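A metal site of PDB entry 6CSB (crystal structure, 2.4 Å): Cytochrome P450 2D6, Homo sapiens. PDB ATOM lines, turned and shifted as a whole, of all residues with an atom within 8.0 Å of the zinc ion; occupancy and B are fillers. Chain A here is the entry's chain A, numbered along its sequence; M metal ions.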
ATOM      1  N   ALA A 165      13.927  24.567 -29.172  1.00  0.00           N
ATOM      2  CA  ALA A 165      12.582  24.113 -28.778  1.00  0.00           C
ATOM      3  C   ALA A 165      12.440  22.617 -28.984  1.00  0.00           C
ATOM      4  O   ALA A 165      11.862  21.915 -28.126  1.00  0.00           O
ATOM      5  CB  ALA A 165      11.501  24.866 -29.569  1.00  0.00           C
ATOM      6  N   SER A 166      12.976  22.097 -30.080  1.00  0.00           N
ATOM      7  CA  SER A 166      12.912  20.661 -30.337  1.00  0.00           C
ATOM      8  C   SER A 166      13.700  19.896 -29.281  1.00  0.00           C
ATOM      9  O   SER A 166      13.208  18.904 -28.733  1.00  0.00           O
ATOM     10  CB  SER A 166      13.448  20.320 -31.727  1.00  0.00           C
ATOM     11  OG  SER A 166      12.701  20.985 -32.715  1.00  0.00           O
ATOM     12  N   LEU A 167      14.944  20.314 -29.035  1.00  0.00           N
ATOM     13  CA  LEU A 167      15.780  19.689 -28.023  1.00  0.00           C
ATOM     14  C   LEU A 167      15.093  19.684 -26.666  1.00  0.00           C
ATOM     15  O   LEU A 167      15.070  18.664 -25.964  1.00  0.00           O
ATOM     16  CB  LEU A 167      17.128  20.440 -27.935  1.00  0.00           C
ATOM     17  CG  LEU A 167      17.908  20.287 -26.603  1.00  0.00           C
ATOM     18  CD1 LEU A 167      18.415  18.870 -26.418  1.00  0.00           C
ATOM     19  CD2 LEU A 167      19.061  21.272 -26.471  1.00  0.00           C
ATOM     20  N   THR A 168      14.536  20.826 -26.279  1.00  0.00           N
ATOM     21  CA  THR A 168      14.082  20.989 -24.918  1.00  0.00           C
ATOM     22  C   THR A 168      12.613  20.645 -24.733  1.00  0.00           C
ATOM     23  O   THR A 168      12.260  20.138 -23.670  1.00  0.00           O
ATOM     24  CB  THR A 168      14.343  22.419 -24.447  1.00  0.00           C
ATOM     25  OG1 THR A 168      13.539  23.313 -25.216  1.00  0.00           O
ATOM     26  CG2 THR A 168      15.825  22.786 -24.606  1.00  0.00           C
ATOM     27  N   CYS A 169      11.747  20.883 -25.714  1.00  0.00           N
ATOM     28  CA  CYS A 169      10.322  20.596 -25.541  1.00  0.00           C
ATOM     29  C   CYS A 169       9.734  19.653 -26.576  1.00  0.00           C
ATOM     30  O   CYS A 169       8.533  19.383 -26.516  1.00  0.00           O
ATOM     31  CB  CYS A 169       9.503  21.893 -25.550  1.00  0.00           C
ATOM     32  SG  CYS A 169       9.833  22.979 -24.160  1.00  0.00           S
ATOM     33  N   GLY A 170      10.519  19.162 -27.536  1.00  0.00           N
ATOM     34  CA  GLY A 170       9.990  18.217 -28.496  1.00  0.00           C
ATOM     35  C   GLY A 170       8.998  18.762 -29.500  1.00  0.00           C
ATOM     36  O   GLY A 170       8.227  17.996 -30.077  1.00  0.00           O
ATOM     37  N   ARG A 171       9.010  20.065 -29.758  1.00  0.00           N
ATOM     38  CA  ARG A 171       8.151  20.666 -30.768  1.00  0.00           C
ATOM     39  C   ARG A 171       8.930  21.743 -31.510  1.00  0.00           C
ATOM     40  O   ARG A 171      10.038  22.129 -31.098  1.00  0.00           O
ATOM     41  CB  ARG A 171       6.888  21.282 -30.121  1.00  0.00           C
ATOM     42  CG  ARG A 171       7.176  22.457 -29.209  1.00  0.00           C
ATOM     43  CD  ARG A 171       5.930  23.290 -28.956  1.00  0.00           C
ATOM     44  NE  ARG A 171       5.343  23.730 -30.217  1.00  0.00           N
ATOM     45  CZ  ARG A 171       4.162  24.325 -30.340  1.00  0.00           C
ATOM     46  NH1 ARG A 171       3.395  24.568 -29.266  1.00  0.00           N
ATOM     47  NH2 ARG A 171       3.742  24.672 -31.551  1.00  0.00           N
ATOM     48  N   HIS A 236       3.867  21.558 -21.903  1.00  0.00           N
ATOM     49  CA  HIS A 236       4.608  20.329 -22.144  1.00  0.00           C
ATOM     50  C   HIS A 236       4.360  19.331 -21.016  1.00  0.00           C
ATOM     51  O   HIS A 236       4.253  18.124 -21.251  1.00  0.00           O
ATOM     52  CB  HIS A 236       6.109  20.623 -22.291  1.00  0.00           C
ATOM     53  CG  HIS A 236       6.902  19.463 -22.823  1.00  0.00           C
ATOM     54  ND1 HIS A 236       8.278  19.403 -22.782  1.00  0.00           N
ATOM     55  CD2 HIS A 236       6.512  18.319 -23.438  1.00  0.00           C
ATOM     56  CE1 HIS A 236       8.698  18.298 -23.345  1.00  0.00           C
ATOM     57  NE2 HIS A 236       7.656  17.615 -23.755  1.00  0.00           N
ATOM     58  N   ARG A 237       4.234  19.833 -19.788  1.00  0.00           N
ATOM     59  CA  ARG A 237       3.917  18.957 -18.670  1.00  0.00           C
ATOM     60  C   ARG A 237       2.640  18.183 -18.935  1.00  0.00           C
ATOM     61  O   ARG A 237       2.542  17.002 -18.601  1.00  0.00           O
ATOM     62  CB  ARG A 237       3.786  19.787 -17.406  1.00  0.00           C
ATOM     63  CG  ARG A 237       4.533  19.250 -16.218  1.00  0.00           C
ATOM     64  CD  ARG A 237       4.699  20.327 -15.170  1.00  0.00           C
ATOM     65  NE  ARG A 237       5.511  19.858 -14.062  1.00  0.00           N
ATOM     66  CZ  ARG A 237       6.554  20.530 -13.577  1.00  0.00           C
ATOM     67  NH1 ARG A 237       6.890  21.705 -14.101  1.00  0.00           N
ATOM     68  NH2 ARG A 237       7.241  20.017 -12.566  1.00  0.00           N
ATOM     69  N   THR A 239       1.330  17.231 -21.863  1.00  0.00           N
ATOM     70  CA  THR A 239       1.388  16.242 -22.946  1.00  0.00           C
ATOM     71  C   THR A 239       2.446  15.165 -22.724  1.00  0.00           C
ATOM     72  O   THR A 239       2.505  14.211 -23.517  1.00  0.00           O
ATOM     73  CB  THR A 239       1.649  16.904 -24.285  1.00  0.00           C
ATOM     74  OG1 THR A 239       2.879  17.634 -24.210  1.00  0.00           O
ATOM     75  CG2 THR A 239       0.514  17.855 -24.633  1.00  0.00           C
ATOM     76  N   TRP A 240       3.265  15.292 -21.689  1.00  0.00           N
ATOM     77  CA  TRP A 240       4.313  14.325 -21.437  1.00  0.00           C
ATOM     78  C   TRP A 240       3.722  12.954 -21.115  1.00  0.00           C
ATOM     79  O   TRP A 240       2.791  12.833 -20.310  1.00  0.00           O
ATOM     80  CB  TRP A 240       5.192  14.804 -20.289  1.00  0.00           C
ATOM     81  CG  TRP A 240       6.179  13.819 -19.794  1.00  0.00           C
ATOM     82  CD1 TRP A 240       6.908  12.922 -20.524  1.00  0.00           C
ATOM     83  CD2 TRP A 240       6.540  13.622 -18.432  1.00  0.00           C
ATOM     84  NE1 TRP A 240       7.709  12.175 -19.686  1.00  0.00           N
ATOM     85  CE2 TRP A 240       7.510  12.601 -18.403  1.00  0.00           C
ATOM     86  CE3 TRP A 240       6.152  14.231 -17.232  1.00  0.00           C
ATOM     87  CZ2 TRP A 240       8.096  12.162 -17.206  1.00  0.00           C
ATOM     88  CZ3 TRP A 240       6.722  13.775 -16.039  1.00  0.00           C
ATOM     89  CH2 TRP A 240       7.701  12.764 -16.049  1.00  0.00           C
ATOM     90  N   ASP A 241       4.263  11.924 -21.759  1.00  0.00           N
ATOM     91  CA  ASP A 241       3.833  10.547 -21.534  1.00  0.00           C
ATOM     92  C   ASP A 241       4.937   9.829 -20.772  1.00  0.00           C
ATOM     93  O   ASP A 241       5.856   9.275 -21.401  1.00  0.00           O
ATOM     94  CB  ASP A 241       3.536   9.848 -22.860  1.00  0.00           C
ATOM     95  CG  ASP A 241       2.968   8.473 -22.664  1.00  0.00           C
ATOM     96  OD1 ASP A 241       2.854   8.047 -21.497  1.00  0.00           O
ATOM     97  OD2 ASP A 241       2.615   7.821 -23.676  1.00  0.00           O
ATOM     98  N   PRO A 245       9.811   6.330 -23.164  1.00  0.00           N
ATOM     99  CA  PRO A 245      11.108   6.943 -22.944  1.00  0.00           C
ATOM    100  C   PRO A 245      11.048   8.427 -23.264  1.00  0.00           C
ATOM    101  O   PRO A 245      10.281   8.856 -24.151  1.00  0.00           O
ATOM    102  CB  PRO A 245      12.018   6.197 -23.939  1.00  0.00           C
ATOM    103  CG  PRO A 245      11.309   4.911 -24.200  1.00  0.00           C
ATOM    104  CD  PRO A 245       9.865   5.275 -24.191  1.00  0.00           C
ATOM    105  N   PRO A 246      11.811   9.242 -22.543  1.00  0.00           N
ATOM    106  CA  PRO A 246      11.741  10.694 -22.768  1.00  0.00           C
ATOM    107  C   PRO A 246      12.091  11.024 -24.211  1.00  0.00           C
ATOM    108  O   PRO A 246      13.033  10.472 -24.786  1.00  0.00           O
ATOM    109  CB  PRO A 246      12.763  11.262 -21.784  1.00  0.00           C
ATOM    110  CG  PRO A 246      13.101  10.140 -20.847  1.00  0.00           C
ATOM    111  CD  PRO A 246      12.909   8.888 -21.631  1.00  0.00           C
ATOM    112  N   ARG A 247      11.315  11.902 -24.811  1.00  0.00           N
ATOM    113  CA  ARG A 247      11.598  12.212 -26.198  1.00  0.00           C
ATOM    114  C   ARG A 247      12.339  13.530 -26.351  1.00  0.00           C
ATOM    115  O   ARG A 247      12.667  13.911 -27.470  1.00  0.00           O
ATOM    116  CB  ARG A 247      10.305  12.192 -27.023  1.00  0.00           C
ATOM    117  CG  ARG A 247       9.195  13.110 -26.556  1.00  0.00           C
ATOM    118  CD  ARG A 247       8.019  13.022 -27.535  1.00  0.00           C
ATOM    119  NE  ARG A 247       8.484  13.074 -28.930  1.00  0.00           N
ATOM    120  CZ  ARG A 247       8.574  14.184 -29.657  1.00  0.00           C
ATOM    121  NH1 ARG A 247       8.217  15.355 -29.156  1.00  0.00           N
ATOM    122  NH2 ARG A 247       9.025  14.117 -30.908  1.00  0.00           N
ATOM    123  N   ASP A 248      12.644  14.213 -25.252  1.00  0.00           N
ATOM    124  CA  ASP A 248      13.349  15.482 -25.303  1.00  0.00           C
ATOM    125  C   ASP A 248      13.918  15.779 -23.909  1.00  0.00           C
ATOM    126  O   ASP A 248      13.716  15.035 -22.954  1.00  0.00           O
ATOM    127  CB  ASP A 248      12.415  16.571 -25.799  1.00  0.00           C
ATOM    128  CG  ASP A 248      11.114  16.618 -24.996  1.00  0.00           C
ATOM    129  OD1 ASP A 248      11.182  16.730 -23.748  1.00  0.00           O
ATOM    130  OD2 ASP A 248      10.029  16.502 -25.609  1.00  0.00           O
ATOM    131  N   LEU A 249      14.606  16.906 -23.790  1.00  0.00           N
ATOM    132  CA  LEU A 249      15.424  17.079 -22.605  1.00  0.00           C
ATOM    133  C   LEU A 249      14.547  17.349 -21.403  1.00  0.00           C
ATOM    134  O   LEU A 249      14.824  16.839 -20.304  1.00  0.00           O
ATOM    135  CB  LEU A 249      16.446  18.211 -22.835  1.00  0.00           C
ATOM    136  CG  LEU A 249      17.356  18.590 -21.655  1.00  0.00           C
ATOM    137  CD1 LEU A 249      18.782  18.927 -22.148  1.00  0.00           C
ATOM    138  CD2 LEU A 249      16.743  19.747 -20.886  1.00  0.00           C
ATOM    139  N   THR A 250      13.491  18.104 -21.591  1.00  0.00           N
ATOM    140  CA  THR A 250      12.625  18.417 -20.465  1.00  0.00           C
ATOM    141  C   THR A 250      11.944  17.171 -19.915  1.00  0.00           C
ATOM    142  O   THR A 250      11.744  17.041 -18.710  1.00  0.00           O
ATOM    143  CB  THR A 250      11.607  19.460 -20.898  1.00  0.00           C
ATOM    144  OG1 THR A 250      12.240  20.733 -20.843  1.00  0.00           O
ATOM    145  CG2 THR A 250      10.376  19.434 -20.016  1.00  0.00           C
ATOM    146  N   GLU A 251      11.609  16.230 -20.782  1.00  0.00           N
ATOM    147  CA  GLU A 251      11.039  14.978 -20.287  1.00  0.00           C
ATOM    148  C   GLU A 251      12.071  14.206 -19.479  1.00  0.00           C
ATOM    149  O   GLU A 251      11.792  13.774 -18.343  1.00  0.00           O
ATOM    150  CB  GLU A 251      10.504  14.144 -21.468  1.00  0.00           C
ATOM    151  CG  GLU A 251       9.228  14.755 -22.087  1.00  0.00           C
ATOM    152  CD  GLU A 251       8.620  13.925 -23.210  1.00  0.00           C
ATOM    153  OE1 GLU A 251       8.969  12.726 -23.324  1.00  0.00           O
ATOM    154  OE2 GLU A 251       7.821  14.470 -23.977  1.00  0.00           O
ATOM    155  N   ALA A 252      13.274  14.032 -20.024  1.00  0.00           N
ATOM    156  CA  ALA A 252      14.364  13.400 -19.271  1.00  0.00           C
ATOM    157  C   ALA A 252      14.506  14.052 -17.911  1.00  0.00           C
ATOM    158  O   ALA A 252      14.611  13.367 -16.875  1.00  0.00           O
ATOM    159  CB  ALA A 252      15.670  13.500 -20.081  1.00  0.00           C
ATOM    160  N   LEU A 254      12.212  15.835 -16.215  1.00  0.00           N
ATOM    161  CA  LEU A 254      11.044  15.573 -15.382  1.00  0.00           C
ATOM    162  C   LEU A 254      11.096  14.166 -14.792  1.00  0.00           C
ATOM    163  O   LEU A 254      10.738  13.955 -13.628  1.00  0.00           O
ATOM    164  CB  LEU A 254       9.770  15.775 -16.198  1.00  0.00           C
ATOM    165  CG  LEU A 254       9.389  17.233 -16.484  1.00  0.00           C
ATOM    166  CD1 LEU A 254       8.355  17.282 -17.605  1.00  0.00           C
ATOM    167  CD2 LEU A 254       8.867  17.966 -15.247  1.00  0.00           C
HETATM  168 ZN    ZN M   1       8.121  16.253 -24.856  1.00  0.00          ZN
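The zinc ion is bound by NE2 of His 236 (1.8 Å), OE2 of Glu 251 (2.0 Å) and OD2 of Asp 248 (2.1 Å).
Residues that only touch the zinc ion: Cys 169 and Arg 247. Of the 21 residues printed, 5 come within 4 Å of the zinc ion. The nearest printed residue that does not touch the zinc ion is Gly 170 (4.5 Å).
The backbone carbonyl oxygen of Cys 169 lies close to a ring nitrogen (NE2) of His 236. O of His 236 sits at hydrogen-bond distance from OG1 of Thr 239. OE1 of Glu 251 is in hydrogen-bond range of N of Arg 247 (2.9 Å). The side-chain carboxylate (OD2) of Asp 248 sits close to the backbone NH (N) of Gly 170, at 3.3 Å. The side-chain carboxylate of Asp 248 sits close to the backbone NH of Thr 250, 3.4 Å away. The guanidinium group (NH1) of Arg 247 is in hydrogen-bond range of the backbone carbonyl oxygen (O) of Gly 170, at 2.8 Å.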
